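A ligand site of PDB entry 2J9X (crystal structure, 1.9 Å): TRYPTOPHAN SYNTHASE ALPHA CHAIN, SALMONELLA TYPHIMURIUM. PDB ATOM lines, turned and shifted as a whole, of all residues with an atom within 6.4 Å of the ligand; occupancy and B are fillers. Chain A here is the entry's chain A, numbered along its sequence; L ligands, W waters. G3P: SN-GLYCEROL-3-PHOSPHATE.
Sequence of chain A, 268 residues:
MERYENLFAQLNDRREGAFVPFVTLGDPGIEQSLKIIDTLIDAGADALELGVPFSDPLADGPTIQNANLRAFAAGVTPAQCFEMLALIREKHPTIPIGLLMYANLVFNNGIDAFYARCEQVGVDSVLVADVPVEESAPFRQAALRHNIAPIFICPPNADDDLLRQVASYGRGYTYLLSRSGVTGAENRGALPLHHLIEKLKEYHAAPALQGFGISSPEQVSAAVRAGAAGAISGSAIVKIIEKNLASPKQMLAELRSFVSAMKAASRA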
ATOM      1  N   PHE A  22     -14.663  -3.366 -20.205  1.00  0.00           N
ATOM      2  CA  PHE A  22     -15.236  -2.309 -19.372  1.00  0.00           C
ATOM      3  C   PHE A  22     -14.146  -1.422 -18.812  1.00  0.00           C
ATOM      4  O   PHE A  22     -13.106  -1.905 -18.376  1.00  0.00           O
ATOM      5  CB  PHE A  22     -16.049  -2.867 -18.199  1.00  0.00           C
ATOM      6  CG  PHE A  22     -16.404  -1.830 -17.155  1.00  0.00           C
ATOM      7  CD1 PHE A  22     -15.457  -1.389 -16.230  1.00  0.00           C
ATOM      8  CD2 PHE A  22     -17.677  -1.249 -17.127  1.00  0.00           C
ATOM      9  CE1 PHE A  22     -15.764  -0.387 -15.303  1.00  0.00           C
ATOM     10  CE2 PHE A  22     -17.986  -0.252 -16.208  1.00  0.00           C
ATOM     11  CZ  PHE A  22     -17.031   0.186 -15.295  1.00  0.00           C
ATOM     12  N   GLU A  49     -18.771  -1.385 -22.506  1.00  0.00           N
ATOM     13  CA  GLU A  49     -19.483  -1.308 -21.235  1.00  0.00           C
ATOM     14  C   GLU A  49     -18.718  -0.195 -20.536  1.00  0.00           C
ATOM     15  O   GLU A  49     -17.543  -0.348 -20.229  1.00  0.00           O
ATOM     16  CB  GLU A  49     -19.328  -2.611 -20.457  1.00  0.00           C
ATOM     17  CG  GLU A  49     -20.250  -2.733 -19.266  1.00  0.00           C
ATOM     18  CD  GLU A  49     -21.675  -3.023 -19.691  1.00  0.00           C
ATOM     19  OE1 GLU A  49     -22.512  -3.256 -18.800  1.00  0.00           O
ATOM     20  OE2 GLU A  49     -21.947  -3.028 -20.903  1.00  0.00           O
ATOM     21  N   ASP A  60     -18.698  -2.253  -6.694  1.00  0.00           N
ATOM     22  CA  ASP A  60     -17.323  -2.362  -7.157  1.00  0.00           C
ATOM     23  C   ASP A  60     -16.293  -2.632  -6.076  1.00  0.00           C
ATOM     24  O   ASP A  60     -16.403  -2.158  -4.949  1.00  0.00           O
ATOM     25  CB  ASP A  60     -16.942  -1.101  -7.937  1.00  0.00           C
ATOM     26  CG  ASP A  60     -17.621  -1.032  -9.286  1.00  0.00           C
ATOM     27  OD1 ASP A  60     -17.304  -1.879 -10.148  1.00  0.00           O
ATOM     28  OD2 ASP A  60     -18.480  -0.144  -9.484  1.00  0.00           O
ATOM     29  N   ILE A  64     -11.799  -0.969  -9.475  1.00  0.00           N
ATOM     30  CA  ILE A  64     -12.671   0.026 -10.080  1.00  0.00           C
ATOM     31  C   ILE A  64     -12.949   1.210  -9.169  1.00  0.00           C
ATOM     32  O   ILE A  64     -13.333   2.277  -9.626  1.00  0.00           O
ATOM     33  CB  ILE A  64     -13.972  -0.636 -10.554  1.00  0.00           C
ATOM     34  CG1 ILE A  64     -13.655  -1.663 -11.636  1.00  0.00           C
ATOM     35  CG2 ILE A  64     -14.918   0.423 -11.095  1.00  0.00           C
ATOM     36  CD1 ILE A  64     -14.852  -2.332 -12.229  1.00  0.00           C
ATOM     37  N   LEU A 100     -22.837   1.476 -17.451  1.00  0.00           N
ATOM     38  CA  LEU A 100     -23.070   0.806 -16.178  1.00  0.00           C
ATOM     39  C   LEU A 100     -23.149   1.957 -15.189  1.00  0.00           C
ATOM     40  O   LEU A 100     -22.138   2.573 -14.872  1.00  0.00           O
ATOM     41  CB  LEU A 100     -21.918  -0.149 -15.845  1.00  0.00           C
ATOM     42  CG  LEU A 100     -22.208  -1.086 -14.677  1.00  0.00           C
ATOM     43  CD1 LEU A 100     -21.240  -2.266 -14.699  1.00  0.00           C
ATOM     44  CD2 LEU A 100     -22.107  -0.304 -13.373  1.00  0.00           C
ATOM     45  N   LEU A 127     -27.353  -0.027 -17.705  1.00  0.00           N
ATOM     46  CA  LEU A 127     -27.482  -0.970 -16.616  1.00  0.00           C
ATOM     47  C   LEU A 127     -27.291  -0.129 -15.352  1.00  0.00           C
ATOM     48  O   LEU A 127     -26.264   0.530 -15.211  1.00  0.00           O
ATOM     49  CB  LEU A 127     -26.381  -2.027 -16.691  1.00  0.00           C
ATOM     50  CG  LEU A 127     -26.455  -3.273 -15.796  1.00  0.00           C
ATOM     51  CD1 LEU A 127     -25.170  -4.055 -15.898  1.00  0.00           C
ATOM     52  CD2 LEU A 127     -26.717  -2.872 -14.370  1.00  0.00           C
ATOM     53  N   TYR A 175     -27.299  -9.301 -18.523  1.00  0.00           N
ATOM     54  CA  TYR A 175     -26.066  -9.362 -17.766  1.00  0.00           C
ATOM     55  C   TYR A 175     -26.117 -10.580 -16.845  1.00  0.00           C
ATOM     56  O   TYR A 175     -26.844 -10.587 -15.855  1.00  0.00           O
ATOM     57  CB  TYR A 175     -25.860  -8.077 -16.955  1.00  0.00           C
ATOM     58  CG  TYR A 175     -24.446  -7.872 -16.473  1.00  0.00           C
ATOM     59  CD1 TYR A 175     -23.856  -8.750 -15.567  1.00  0.00           C
ATOM     60  CD2 TYR A 175     -23.667  -6.806 -16.951  1.00  0.00           C
ATOM     61  CE1 TYR A 175     -22.548  -8.575 -15.134  1.00  0.00           C
ATOM     62  CE2 TYR A 175     -22.354  -6.621 -16.526  1.00  0.00           C
ATOM     63  CZ  TYR A 175     -21.802  -7.515 -15.616  1.00  0.00           C
ATOM     64  OH  TYR A 175     -20.506  -7.367 -15.175  1.00  0.00           O
ATOM     65  N   ARG A 179     -20.681 -14.487 -10.310  1.00  0.00           N
ATOM     66  CA  ARG A 179     -20.667 -14.826  -8.892  1.00  0.00           C
ATOM     67  C   ARG A 179     -21.284 -13.721  -8.049  1.00  0.00           C
ATOM     68  O   ARG A 179     -21.721 -12.687  -8.561  1.00  0.00           O
ATOM     69  CB  ARG A 179     -19.218 -14.996  -8.433  1.00  0.00           C
ATOM     70  CG  ARG A 179     -18.349 -13.778  -8.771  1.00  0.00           C
ATOM     71  CD  ARG A 179     -16.987 -13.837  -8.118  1.00  0.00           C
ATOM     72  NE  ARG A 179     -16.144 -12.736  -8.569  1.00  0.00           N
ATOM     73  CZ  ARG A 179     -16.331 -11.457  -8.253  1.00  0.00           C
ATOM     74  NH1 ARG A 179     -17.349 -11.097  -7.488  1.00  0.00           N
ATOM     75  NH2 ARG A 179     -15.516 -10.530  -8.741  1.00  0.00           N
ATOM     76  N   VAL A 182     -18.585  -8.205  -5.286  1.00  0.00           N
ATOM     77  CA  VAL A 182     -18.403  -6.995  -6.052  1.00  0.00           C
ATOM     78  C   VAL A 182     -17.397  -7.264  -7.166  1.00  0.00           C
ATOM     79  O   VAL A 182     -16.752  -8.308  -7.184  1.00  0.00           O
ATOM     80  CB  VAL A 182     -17.871  -5.849  -5.171  1.00  0.00           C
ATOM     81  CG1 VAL A 182     -18.907  -5.485  -4.129  1.00  0.00           C
ATOM     82  CG2 VAL A 182     -16.575  -6.275  -4.508  1.00  0.00           C
ATOM     83  N   THR A 183     -17.278  -6.310  -8.079  1.00  0.00           N
ATOM     84  CA  THR A 183     -16.353  -6.422  -9.200  1.00  0.00           C
ATOM     85  C   THR A 183     -14.947  -6.695  -8.666  1.00  0.00           C
ATOM     86  O   THR A 183     -14.575  -6.189  -7.606  1.00  0.00           O
ATOM     87  CB  THR A 183     -16.333  -5.139 -10.027  1.00  0.00           C
ATOM     88  OG1 THR A 183     -15.937  -4.043  -9.203  1.00  0.00           O
ATOM     89  CG2 THR A 183     -17.709  -4.864 -10.603  1.00  0.00           C
ATOM     90  N   GLY A 184     -14.183  -7.483  -9.414  1.00  0.00           N
ATOM     91  CA  GLY A 184     -12.824  -7.814  -9.004  1.00  0.00           C
ATOM     92  C   GLY A 184     -12.283  -8.925  -9.880  1.00  0.00           C
ATOM     93  O   GLY A 184     -12.918  -9.979 -10.010  1.00  0.00           O
ATOM     94  N   ALA A 185     -11.119  -8.689 -10.481  1.00  0.00           N
ATOM     95  CA  ALA A 185     -10.480  -9.659 -11.369  1.00  0.00           C
ATOM     96  C   ALA A 185      -9.926 -10.860 -10.618  1.00  0.00           C
ATOM     97  O   ALA A 185      -9.994 -11.987 -11.106  1.00  0.00           O
ATOM     98  CB  ALA A 185      -9.351  -8.974 -12.141  1.00  0.00           C
ATOM     99  N   ASN A 187     -11.091 -12.360  -8.107  1.00  0.00           N
ATOM    100  CA  ASN A 187     -12.153 -13.272  -7.689  1.00  0.00           C
ATOM    101  C   ASN A 187     -12.814 -13.912  -8.910  1.00  0.00           C
ATOM    102  O   ASN A 187     -13.635 -13.285  -9.581  1.00  0.00           O
ATOM    103  CB  ASN A 187     -13.206 -12.513  -6.881  1.00  0.00           C
ATOM    104  CG  ASN A 187     -14.090 -13.435  -6.072  1.00  0.00           C
ATOM    105  OD1 ASN A 187     -14.355 -14.567  -6.469  1.00  0.00           O
ATOM    106  ND2 ASN A 187     -14.562 -12.939  -4.931  1.00  0.00           N
ATOM    107  N   GLY A 211     -20.447 -11.557 -16.688  1.00  0.00           N
ATOM    108  CA  GLY A 211     -19.601 -10.541 -16.092  1.00  0.00           C
ATOM    109  C   GLY A 211     -19.259 -10.740 -14.621  1.00  0.00           C
ATOM    110  O   GLY A 211     -20.023 -11.371 -13.889  1.00  0.00           O
ATOM    111  N   PHE A 212     -18.126 -10.170 -14.207  1.00  0.00           N
ATOM    112  CA  PHE A 212     -17.597 -10.260 -12.835  1.00  0.00           C
ATOM    113  C   PHE A 212     -16.556 -11.361 -12.763  1.00  0.00           C
ATOM    114  O   PHE A 212     -16.884 -12.530 -12.958  1.00  0.00           O
ATOM    115  CB  PHE A 212     -18.699 -10.554 -11.806  1.00  0.00           C
ATOM    116  CG  PHE A 212     -19.332  -9.327 -11.235  1.00  0.00           C
ATOM    117  CD1 PHE A 212     -19.806  -8.312 -12.067  1.00  0.00           C
ATOM    118  CD2 PHE A 212     -19.490  -9.196  -9.861  1.00  0.00           C
ATOM    119  CE1 PHE A 212     -20.411  -7.176 -11.524  1.00  0.00           C
ATOM    120  CE2 PHE A 212     -20.091  -8.069  -9.313  1.00  0.00           C
ATOM    121  CZ  PHE A 212     -20.556  -7.051 -10.149  1.00  0.00           C
ATOM    122  N   GLY A 213     -15.313 -10.999 -12.493  1.00  0.00           N
ATOM    123  CA  GLY A 213     -14.270 -12.009 -12.374  1.00  0.00           C
ATOM    124  C   GLY A 213     -13.663 -12.535 -13.658  1.00  0.00           C
ATOM    125  O   GLY A 213     -12.705 -13.303 -13.614  1.00  0.00           O
ATOM    126  N   ILE A 214     -14.221 -12.167 -14.812  1.00  0.00           N
ATOM    127  CA  ILE A 214     -13.679 -12.611 -16.093  1.00  0.00           C
ATOM    128  C   ILE A 214     -12.373 -11.845 -16.364  1.00  0.00           C
ATOM    129  O   ILE A 214     -12.425 -10.667 -16.713  1.00  0.00           O
ATOM    130  CB  ILE A 214     -14.675 -12.315 -17.245  1.00  0.00           C
ATOM    131  CG1 ILE A 214     -16.040 -12.914 -16.942  1.00  0.00           C
ATOM    132  CG2 ILE A 214     -14.140 -12.879 -18.554  1.00  0.00           C
ATOM    133  CD1 ILE A 214     -16.038 -14.410 -16.919  1.00  0.00           C
ATOM    134  N   SER A 215     -11.229 -12.504 -16.226  1.00  0.00           N
ATOM    135  CA  SER A 215      -9.944 -11.832 -16.444  1.00  0.00           C
ATOM    136  C   SER A 215      -8.924 -12.639 -17.264  1.00  0.00           C
ATOM    137  O   SER A 215      -7.754 -12.256 -17.323  1.00  0.00           O
ATOM    138  CB  SER A 215      -9.332 -11.444 -15.098  1.00  0.00           C
ATOM    139  OG  SER A 215      -9.129 -12.574 -14.259  1.00  0.00           O
ATOM    140  N   ILE A 232     -17.934 -10.124 -20.422  1.00  0.00           N
ATOM    141  CA  ILE A 232     -17.523  -8.755 -20.106  1.00  0.00           C
ATOM    142  C   ILE A 232     -16.358  -8.821 -19.132  1.00  0.00           C
ATOM    143  O   ILE A 232     -16.364  -9.628 -18.211  1.00  0.00           O
ATOM    144  CB  ILE A 232     -18.688  -7.964 -19.472  1.00  0.00           C
ATOM    145  CG1 ILE A 232     -19.870  -7.936 -20.432  1.00  0.00           C
ATOM    146  CG2 ILE A 232     -18.245  -6.528 -19.133  1.00  0.00           C
ATOM    147  CD1 ILE A 232     -21.115  -7.391 -19.829  1.00  0.00           C
ATOM    148  N   SER A 233     -15.367  -7.962 -19.347  1.00  0.00           N
ATOM    149  CA  SER A 233     -14.195  -7.915 -18.484  1.00  0.00           C
ATOM    150  C   SER A 233     -13.917  -6.463 -18.132  1.00  0.00           C
ATOM    151  O   SER A 233     -13.734  -5.629 -19.023  1.00  0.00           O
ATOM    152  CB  SER A 233     -12.982  -8.517 -19.202  1.00  0.00           C
ATOM    153  OG  SER A 233     -11.874  -8.587 -18.336  1.00  0.00           O
ATOM    154  N   GLY A 234     -13.911  -6.165 -16.844  1.00  0.00           N
ATOM    155  CA  GLY A 234     -13.661  -4.797 -16.420  1.00  0.00           C
ATOM    156  C   GLY A 234     -12.383  -4.617 -15.612  1.00  0.00           C
ATOM    157  O   GLY A 234     -11.432  -3.994 -16.088  1.00  0.00           O
ATOM    158  N   SER A 235     -12.367  -5.167 -14.405  1.00  0.00           N
ATOM    159  CA  SER A 235     -11.213  -5.058 -13.508  1.00  0.00           C
ATOM    160  C   SER A 235      -9.888  -5.466 -14.117  1.00  0.00           C
ATOM    161  O   SER A 235      -8.869  -4.827 -13.853  1.00  0.00           O
ATOM    162  CB  SER A 235     -11.464  -5.870 -12.247  1.00  0.00           C
ATOM    163  OG  SER A 235     -12.507  -5.307 -11.480  1.00  0.00           O
ATOM    164  N   ALA A 236      -9.900  -6.532 -14.908  1.00  0.00           N
ATOM    165  CA  ALA A 236      -8.676  -7.010 -15.552  1.00  0.00           C
ATOM    166  C   ALA A 236      -8.127  -5.924 -16.470  1.00  0.00           C
ATOM    167  O   ALA A 236      -6.910  -5.715 -16.541  1.00  0.00           O
ATOM    168  CB  ALA A 236      -8.959  -8.271 -16.344  1.00  0.00           C
HETATM  169  O1  G3P L   1     -19.490  -4.882 -15.877  1.00  0.00           O
HETATM  170  C1  G3P L   1     -18.059  -4.784 -15.761  1.00  0.00           C
HETATM  171  C2  G3P L   1     -17.681  -4.835 -14.284  1.00  0.00           C
HETATM  172  O2  G3P L   1     -16.537  -4.153 -13.837  1.00  0.00           O
HETATM  173  C3  G3P L   1     -17.525  -6.322 -13.795  1.00  0.00           C
HETATM  174  O1P G3P L   1     -16.670  -6.926 -14.243  1.00  0.00           O
HETATM  175  O4P G3P L   1     -15.573  -8.017 -12.134  1.00  0.00           O
HETATM  176  O2P G3P L   1     -14.601  -5.920 -13.008  1.00  0.00           O
HETATM  177  O3P G3P L   1     -14.309  -8.056 -14.305  1.00  0.00           O
HETATM  178  P   G3P L   1     -15.283  -7.237 -13.439  1.00  0.00           P
HETATM  179  O   HOH W   1     -16.104  -9.726 -15.588  1.00  0.00           O
HETATM  180  O   HOH W   2     -11.816  -8.561 -14.740  1.00  0.00           O
HETATM  181  O   HOH W   3     -18.535  -2.068 -12.586  1.00  0.00           O
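The backbone NH (N) of Gly 213 lies within hydrogen-bond range of an oxygen (O4P) of the ligand (3.0 Å).
An oxygen (O2P) of the ligand lies within hydrogen-bond range of the backbone NH (N) of Ser 235 (2.7 Å).
O1 of the ligand lies within hydrogen-bond range of OH of Tyr 175 (2.8 Å).
O2P of the ligand sits at hydrogen-bond distance from OG of Ser 235, at 2.7 Å.
N of Gly 234 sits at hydrogen-bond distance from O3P of the ligand (3.2 Å).
N of Gly 184 is in hydrogen-bond range of O4P of the ligand, at 3.1 Å.
The backbone carbonyl oxygen (O) of Gly 184 sits at hydrogen-bond distance from the guanidinium group (NH2) of Arg 179, 2.9 Å away.
The backbone NH (N) of Phe 22 sits at hydrogen-bond distance from the backbone carbonyl oxygen (O) of Ser 233.
The side-chain hydroxyl (OG1) of Thr 183 lies within hydrogen-bond range of the side-chain carboxylate (OD1) of Asp 60.
N of Gly 184 is in hydrogen-bond range of OG of Ser 235 (3.4 Å).
Merely in contact with the ligand: Ile 64, Phe 212, Leu 100, Thr 183, Phe 22 and Ile 232.
11 residues have an atom within 4 Å of the ligand: Phe 22, Ile 64, Leu 100, Tyr 175, Thr 183, Gly 184, Phe 212, Gly 213, Ile 232, Gly 234 and Ser 235.
Along chain A the residues within 4 Å of the ligand span positions 22 to 235.
The nearest printed residue that does not touch the ligand is Ile 214 (4.02 Å).
Water W2 lies within hydrogen-bond range of O3P of the ligand (2.6 Å), N of Ala 236 (2.8 Å), O of Ile 214 (2.9 Å) and N of Ser 235 (3.5 Å).
Water W3 bridges the side-chain carboxylate (OD1) of Asp 60 (2.7 Å) and an oxygen (O2) of the ligand (3.1 Å).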
